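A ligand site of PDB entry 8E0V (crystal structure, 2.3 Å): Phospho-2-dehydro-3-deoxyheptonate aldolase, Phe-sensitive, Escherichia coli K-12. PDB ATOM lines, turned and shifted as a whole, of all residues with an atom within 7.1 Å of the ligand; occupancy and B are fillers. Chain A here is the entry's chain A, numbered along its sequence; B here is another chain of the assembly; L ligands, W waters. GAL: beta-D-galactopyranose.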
ATOM      1  N   PHE A  96       5.352  34.433   2.783  1.00  0.00           N
ATOM      2  CA  PHE A  96       5.638  33.975   1.427  1.00  0.00           C
ATOM      3  C   PHE A  96       4.390  33.825   0.581  1.00  0.00           C
ATOM      4  O   PHE A  96       4.477  33.795  -0.650  1.00  0.00           O
ATOM      5  CB  PHE A  96       6.421  32.660   1.488  1.00  0.00           C
ATOM      6  CG  PHE A  96       7.722  32.838   2.167  1.00  0.00           C
ATOM      7  CD1 PHE A  96       8.721  33.576   1.554  1.00  0.00           C
ATOM      8  CD2 PHE A  96       7.954  32.301   3.436  1.00  0.00           C
ATOM      9  CE1 PHE A  96       9.941  33.765   2.173  1.00  0.00           C
ATOM     10  CE2 PHE A  96       9.184  32.474   4.092  1.00  0.00           C
ATOM     11  CZ  PHE A  96      10.180  33.209   3.470  1.00  0.00           C
ATOM     12  N   GLU A  97       3.239  33.806   1.220  1.00  0.00           N
ATOM     13  CA  GLU A  97       1.994  33.484   0.547  1.00  0.00           C
ATOM     14  C   GLU A  97       0.868  34.351   1.094  1.00  0.00           C
ATOM     15  O   GLU A  97       0.849  34.698   2.277  1.00  0.00           O
ATOM     16  CB  GLU A  97       1.696  31.974   0.734  1.00  0.00           C
ATOM     17  CG  GLU A  97       0.348  31.616   0.233  1.00  0.00           C
ATOM     18  CD  GLU A  97       0.051  30.134   0.223  1.00  0.00           C
ATOM     19  OE1 GLU A  97       0.822  29.325   0.824  1.00  0.00           O
ATOM     20  OE2 GLU A  97      -0.947  29.797  -0.455  1.00  0.00           O
ATOM     21  N   LYS A 106       0.296  31.538  -5.886  1.00  0.00           N
ATOM     22  CA  LYS A 106       0.320  30.732  -4.638  1.00  0.00           C
ATOM     23  C   LYS A 106       1.516  31.123  -3.758  1.00  0.00           C
ATOM     24  O   LYS A 106       1.781  30.403  -2.804  1.00  0.00           O
ATOM     25  CB  LYS A 106       0.266  29.233  -4.981  1.00  0.00           C
ATOM     26  CG  LYS A 106      -0.868  28.803  -5.896  1.00  0.00           C
ATOM     27  CD  LYS A 106      -2.237  28.975  -5.270  1.00  0.00           C
ATOM     28  N   ILE A 109       6.983  30.254  -1.998  1.00  0.00           N
ATOM     29  CA  ILE A 109       7.420  28.873  -1.799  1.00  0.00           C
ATOM     30  C   ILE A 109       6.846  27.971  -2.885  1.00  0.00           C
ATOM     31  O   ILE A 109       7.577  27.188  -3.501  1.00  0.00           O
ATOM     32  CB  ILE A 109       7.051  28.380  -0.399  1.00  0.00           C
ATOM     33  CG1 ILE A 109       7.887  29.160   0.608  1.00  0.00           C
ATOM     34  CG2 ILE A 109       7.264  26.853  -0.296  1.00  0.00           C
ATOM     35  CD1 ILE A 109       7.571  28.812   2.028  1.00  0.00           C
ATOM     36  N   ASN A 110       5.530  28.121  -3.165  1.00  0.00           N
ATOM     37  CA  ASN A 110       4.830  27.298  -4.148  1.00  0.00           C
ATOM     38  C   ASN A 110       5.368  27.682  -5.508  1.00  0.00           C
ATOM     39  O   ASN A 110       5.769  26.811  -6.291  1.00  0.00           O
ATOM     40  CB  ASN A 110       3.321  27.465  -4.043  1.00  0.00           C
ATOM     41  CG  ASN A 110       2.738  26.784  -2.836  1.00  0.00           C
ATOM     42  OD1 ASN A 110       2.947  25.588  -2.602  1.00  0.00           O
ATOM     43  ND2 ASN A 110       1.994  27.539  -2.041  1.00  0.00           N
ATOM     44  N   PHE A 118       4.637  25.613  -9.942  1.00  0.00           N
ATOM     45  CA  PHE A 118       4.771  24.898  -8.670  1.00  0.00           C
ATOM     46  C   PHE A 118       6.157  24.286  -8.479  1.00  0.00           C
ATOM     47  O   PHE A 118       6.337  23.084  -8.301  1.00  0.00           O
ATOM     48  CB  PHE A 118       3.695  23.826  -8.561  1.00  0.00           C
ATOM     49  CG  PHE A 118       2.492  24.280  -7.764  1.00  0.00           C
ATOM     50  CD1 PHE A 118       2.594  24.437  -6.378  1.00  0.00           C
ATOM     51  CD2 PHE A 118       1.291  24.624  -8.410  1.00  0.00           C
ATOM     52  CE1 PHE A 118       1.504  24.892  -5.622  1.00  0.00           C
ATOM     53  CE2 PHE A 118       0.189  25.079  -7.674  1.00  0.00           C
ATOM     54  CZ  PHE A 118       0.282  25.213  -6.265  1.00  0.00           C
ATOM     55  N   ILE A 120       8.299  23.928  -5.944  1.00  0.00           N
ATOM     56  CA  ILE A 120       8.344  24.073  -4.494  1.00  0.00           C
ATOM     57  C   ILE A 120       9.764  23.911  -3.951  1.00  0.00           C
ATOM     58  O   ILE A 120      10.146  24.569  -2.966  1.00  0.00           O
ATOM     59  CB  ILE A 120       7.381  23.085  -3.809  1.00  0.00           C
ATOM     60  CG1 ILE A 120       5.942  23.521  -4.020  1.00  0.00           C
ATOM     61  CG2 ILE A 120       7.676  22.963  -2.271  1.00  0.00           C
ATOM     62  CD1 ILE A 120       4.956  22.350  -3.953  1.00  0.00           C
ATOM     63  N   LEU A 124      11.462  26.716  -1.625  1.00  0.00           N
ATOM     64  CA  LEU A 124      11.984  26.515  -0.250  1.00  0.00           C
ATOM     65  C   LEU A 124      13.425  27.042  -0.165  1.00  0.00           C
ATOM     66  O   LEU A 124      13.751  27.685   0.829  1.00  0.00           O
ATOM     67  CB  LEU A 124      11.882  25.027   0.108  1.00  0.00           C
ATOM     68  CG  LEU A 124      10.469  24.516   0.362  1.00  0.00           C
ATOM     69  CD1 LEU A 124      10.406  22.996   0.216  1.00  0.00           C
ATOM     70  CD2 LEU A 124       9.963  24.945   1.720  1.00  0.00           C
ATOM     71  N   LEU A 146       1.016  28.337   7.817  1.00  0.00           N
ATOM     72  CA  LEU A 146      -0.200  27.871   7.156  1.00  0.00           C
ATOM     73  C   LEU A 146      -0.354  26.354   7.165  1.00  0.00           C
ATOM     74  O   LEU A 146      -1.477  25.858   7.040  1.00  0.00           O
ATOM     75  CB  LEU A 146      -0.246  28.356   5.704  1.00  0.00           C
ATOM     76  CG  LEU A 146      -0.008  29.860   5.535  1.00  0.00           C
ATOM     77  CD1 LEU A 146       0.034  30.203   4.068  1.00  0.00           C
ATOM     78  CD2 LEU A 146      -1.085  30.694   6.278  1.00  0.00           C
ATOM     79  N   ASP A 147       0.724  25.584   7.309  1.00  0.00           N
ATOM     80  CA  ASP A 147       0.655  24.144   7.158  1.00  0.00           C
ATOM     81  C   ASP A 147       1.641  23.510   8.132  1.00  0.00           C
ATOM     82  O   ASP A 147       2.477  24.197   8.745  1.00  0.00           O
ATOM     83  CB  ASP A 147       0.959  23.728   5.726  1.00  0.00           C
ATOM     84  CG  ASP A 147       2.419  23.970   5.363  1.00  0.00           C
ATOM     85  OD1 ASP A 147       2.774  25.118   5.053  1.00  0.00           O
ATOM     86  OD2 ASP A 147       3.246  23.028   5.450  1.00  0.00           O
ATOM     87  N   MET A 148       1.544  22.183   8.264  1.00  0.00           N
ATOM     88  CA  MET A 148       2.370  21.462   9.214  1.00  0.00           C
ATOM     89  C   MET A 148       3.736  21.014   8.658  1.00  0.00           C
ATOM     90  O   MET A 148       4.549  20.499   9.426  1.00  0.00           O
ATOM     91  CB  MET A 148       1.616  20.258   9.738  1.00  0.00           C
ATOM     92  CG  MET A 148       0.814  20.535  10.978  1.00  0.00           C
ATOM     93  SD  MET A 148      -0.164  22.033  10.878  1.00  0.00           S
ATOM     94  CE  MET A 148      -1.470  21.379   9.850  1.00  0.00           C
ATOM     95  N   ILE A 149       4.028  21.200   7.381  1.00  0.00           N
ATOM     96  CA  ILE A 149       5.254  20.701   6.793  1.00  0.00           C
ATOM     97  C   ILE A 149       6.262  21.827   6.616  1.00  0.00           C
ATOM     98  O   ILE A 149       7.383  21.723   7.128  1.00  0.00           O
ATOM     99  CB  ILE A 149       4.925  19.912   5.513  1.00  0.00           C
ATOM    100  CG1 ILE A 149       4.311  18.571   5.941  1.00  0.00           C
ATOM    101  CG2 ILE A 149       6.151  19.744   4.671  1.00  0.00           C
ATOM    102  CD1 ILE A 149       3.596  17.829   4.888  1.00  0.00           C
ATOM    103  N   THR A 150       5.878  22.915   5.963  1.00  0.00           N
ATOM    104  CA  THR A 150       6.755  24.100   5.722  1.00  0.00           C
ATOM    105  C   THR A 150       7.544  24.569   6.944  1.00  0.00           C
ATOM    106  O   THR A 150       8.698  24.955   6.772  1.00  0.00           O
ATOM    107  CB  THR A 150       5.919  25.271   5.179  1.00  0.00           C
ATOM    108  OG1 THR A 150       5.410  24.893   3.904  1.00  0.00           O
ATOM    109  CG2 THR A 150       6.717  26.558   5.053  1.00  0.00           C
ATOM    110  N   LEU A 154      11.900  26.325   7.992  1.00  0.00           N
ATOM    111  CA  LEU A 154      12.106  27.766   8.162  1.00  0.00           C
ATOM    112  C   LEU A 154      12.028  28.247   9.587  1.00  0.00           C
ATOM    113  O   LEU A 154      12.657  29.258   9.881  1.00  0.00           O
ATOM    114  CB  LEU A 154      11.111  28.578   7.311  1.00  0.00           C
ATOM    115  CG  LEU A 154      10.842  28.090   5.871  1.00  0.00           C
ATOM    116  CD1 LEU A 154       9.682  28.800   5.211  1.00  0.00           C
ATOM    117  CD2 LEU A 154      12.068  28.242   4.998  1.00  0.00           C
ATOM    118  N   MET B 148      -3.738  15.379   9.252  1.00  0.00           N
ATOM    119  CA  MET B 148      -3.138  15.362   7.914  1.00  0.00           C
ATOM    120  C   MET B 148      -2.354  14.077   7.634  1.00  0.00           C
ATOM    121  O   MET B 148      -2.199  13.700   6.470  1.00  0.00           O
ATOM    122  CB  MET B 148      -2.198  16.546   7.722  1.00  0.00           C
ATOM    123  CG  MET B 148      -2.824  17.917   7.555  1.00  0.00           C
ATOM    124  SD  MET B 148      -4.536  17.872   7.056  1.00  0.00           S
ATOM    125  CE  MET B 148      -4.320  17.845   5.274  1.00  0.00           C
ATOM    126  N   GLN B 171      -7.212  25.364   4.745  1.00  0.00           N
ATOM    127  CA  GLN B 171      -6.728  25.102   3.375  1.00  0.00           C
ATOM    128  C   GLN B 171      -6.158  23.694   3.296  1.00  0.00           C
ATOM    129  O   GLN B 171      -6.368  23.055   2.270  1.00  0.00           O
ATOM    130  CB  GLN B 171      -5.693  26.162   2.963  1.00  0.00           C
ATOM    131  CG  GLN B 171      -5.183  26.013   1.544  1.00  0.00           C
ATOM    132  CD  GLN B 171      -6.283  26.198   0.535  1.00  0.00           C
ATOM    133  OE1 GLN B 171      -7.237  26.929   0.768  1.00  0.00           O
ATOM    134  NE2 GLN B 171      -6.154  25.532  -0.592  1.00  0.00           N
ATOM    135  N   VAL B 172      -5.464  23.236   4.337  1.00  0.00           N
ATOM    136  CA  VAL B 172      -4.897  21.907   4.186  1.00  0.00           C
ATOM    137  C   VAL B 172      -5.991  20.865   4.190  1.00  0.00           C
ATOM    138  O   VAL B 172      -5.880  19.823   3.514  1.00  0.00           O
ATOM    139  CB  VAL B 172      -3.808  21.626   5.244  1.00  0.00           C
ATOM    140  CG1 VAL B 172      -2.595  22.587   5.052  1.00  0.00           C
ATOM    141  CG2 VAL B 172      -4.337  21.695   6.654  1.00  0.00           C
ATOM    142  N   GLU B 175      -7.490  20.779   0.783  1.00  0.00           N
ATOM    143  CA  GLU B 175      -6.588  20.080  -0.141  1.00  0.00           C
ATOM    144  C   GLU B 175      -6.752  18.564   0.002  1.00  0.00           C
ATOM    145  O   GLU B 175      -6.921  17.825  -0.997  1.00  0.00           O
ATOM    146  CB  GLU B 175      -5.141  20.495   0.116  1.00  0.00           C
ATOM    147  CG  GLU B 175      -4.762  21.875  -0.517  1.00  0.00           C
ATOM    148  CD  GLU B 175      -3.673  22.568   0.258  1.00  0.00           C
ATOM    149  OE1 GLU B 175      -3.087  21.925   1.177  1.00  0.00           O
ATOM    150  OE2 GLU B 175      -3.401  23.760  -0.035  1.00  0.00           O
ATOM    151  N   CYS B 209      -1.933  21.319  -5.460  1.00  0.00           N
ATOM    152  CA  CYS B 209      -0.550  20.883  -5.410  1.00  0.00           C
ATOM    153  C   CYS B 209      -0.006  21.291  -4.056  1.00  0.00           C
ATOM    154  O   CYS B 209       0.005  22.477  -3.741  1.00  0.00           O
ATOM    155  CB  CYS B 209       0.255  21.530  -6.542  1.00  0.00           C
ATOM    156  SG  CYS B 209       1.994  21.013  -6.578  1.00  0.00           S
ATOM    157  N   PHE B 210       0.426  20.327  -3.253  1.00  0.00           N
ATOM    158  CA  PHE B 210       0.751  20.693  -1.870  1.00  0.00           C
ATOM    159  C   PHE B 210       1.659  19.621  -1.251  1.00  0.00           C
ATOM    160  O   PHE B 210       1.849  18.529  -1.787  1.00  0.00           O
ATOM    161  CB  PHE B 210      -0.520  20.872  -1.031  1.00  0.00           C
ATOM    162  CG  PHE B 210      -1.439  19.689  -1.098  1.00  0.00           C
ATOM    163  CD1 PHE B 210      -2.342  19.540  -2.135  1.00  0.00           C
ATOM    164  CD2 PHE B 210      -1.374  18.683  -0.128  1.00  0.00           C
ATOM    165  CE1 PHE B 210      -3.190  18.402  -2.215  1.00  0.00           C
ATOM    166  CE2 PHE B 210      -2.227  17.555  -0.200  1.00  0.00           C
ATOM    167  CZ  PHE B 210      -3.118  17.402  -1.249  1.00  0.00           C
ATOM    168  N   LEU B 211       2.212  19.964  -0.085  1.00  0.00           N
ATOM    169  CA  LEU B 211       3.079  19.030   0.614  1.00  0.00           C
ATOM    170  C   LEU B 211       2.230  18.091   1.460  1.00  0.00           C
ATOM    171  O   LEU B 211       1.270  18.512   2.095  1.00  0.00           O
ATOM    172  CB  LEU B 211       4.053  19.786   1.506  1.00  0.00           C
ATOM    173  CG  LEU B 211       4.766  20.916   0.801  1.00  0.00           C
ATOM    174  CD1 LEU B 211       5.835  21.407   1.689  1.00  0.00           C
ATOM    175  CD2 LEU B 211       5.333  20.340  -0.475  1.00  0.00           C
ATOM    176  N   SER B 212       2.604  16.816   1.460  1.00  0.00           N
ATOM    177  CA  SER B 212       1.834  15.750   2.079  1.00  0.00           C
ATOM    178  C   SER B 212       2.792  14.597   2.353  1.00  0.00           C
ATOM    179  O   SER B 212       4.007  14.722   2.130  1.00  0.00           O
ATOM    180  CB  SER B 212       0.666  15.328   1.170  1.00  0.00           C
ATOM    181  OG  SER B 212      -0.265  14.462   1.857  1.00  0.00           O
HETATM  182  C1  GAL L   1       0.381  26.018   1.034  1.00  0.00           C
HETATM  183  C2  GAL L   1      -0.430  24.731   1.141  1.00  0.00           C
HETATM  184  C3  GAL L   1       0.245  23.712   2.043  1.00  0.00           C
HETATM  185  C4  GAL L   1       1.730  23.604   1.748  1.00  0.00           C
HETATM  186  C5  GAL L   1       2.363  24.981   1.653  1.00  0.00           C
HETATM  187  C6  GAL L   1       3.812  24.900   1.247  1.00  0.00           C
HETATM  188  O1  GAL L   1      -0.176  26.829   0.012  1.00  0.00           O
HETATM  189  O2  GAL L   1      -1.701  25.060   1.683  1.00  0.00           O
HETATM  190  O3  GAL L   1      -0.374  22.442   1.842  1.00  0.00           O
HETATM  191  O4  GAL L   1       1.911  22.926   0.512  1.00  0.00           O
HETATM  192  O5  GAL L   1       1.703  25.729   0.661  1.00  0.00           O
HETATM  193  O6  GAL L   1       4.438  26.131   1.593  1.00  0.00           O
HETATM  194  O   HOH W   1       0.743  20.700   3.675  1.00  0.00           O
HETATM  195  O   HOH W   2       3.501  28.693   1.221  1.00  0.00           O
HETATM  196  O   HOH W   3       0.763  24.151  -2.143  1.00  0.00           O
HETATM  197  O   HOH W   4      -1.659  27.745  -2.584  1.00  0.00           O
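Water W2 lies within hydrogen-bond range of an oxygen (O6) of the ligand and the side-chain carboxylate of Glu 97.
Water W1 lies within hydrogen-bond range of O of Leu 211 of chain B (2.7 Å) and O3 of the ligand (2.8 Å).
Water W4 bridges OE2 of Glu 97 (3.0 Å) and O1 of the ligand (3.1 Å).
Water W3 lies within hydrogen-bond range of the backbone carbonyl oxygen of Cys 209 of chain B (2.4 Å), the side-chain amide oxygen of Asn 110 (2.7 Å) and an oxygen (O4) of the ligand (3.1 Å).
The side-chain amide nitrogen (ND2) of Asn 110 is in hydrogen-bond range of an oxygen (O1) of the ligand (3.1 Å).
N of Leu 211 of chain B is in hydrogen-bond range of O4 of the ligand (3.0 Å).
The side-chain hydroxyl (OG1) of Thr 150 sits at hydrogen-bond distance from an oxygen (O6) of the ligand.
OE1 of Glu 97 is in hydrogen-bond range of O1 of the ligand.
The side-chain carboxylate of Glu 175 of chain B is in hydrogen-bond range of an oxygen (O2) of the ligand (2.7 Å).
OD2 of Asp 147 is in hydrogen-bond range of N of Thr 150.
OE2 of Glu 175 of chain B sits close to NE2 of Gln 171 of chain B (3.3 Å).
The backbone NH of Ile 149 is in hydrogen-bond range of the side-chain carboxylate of Asp 147 (2.8 Å).
The backbone carbonyl oxygen (O) of Lys 106 is in hydrogen-bond range of the side-chain amide nitrogen (ND2) of Asn 110 (3.0 Å).
Ile 109 touches the ligand.
Asp 147 touches the ligand.
CG of Gln 171 of chain B touches O2 of the ligand, 3.6 Å away.
CG1 of Val 172 of chain B touches O3 of the ligand, at 3.9 Å.
Phe 210 of chain B touches the ligand (CB to O3, 3.3 Å).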
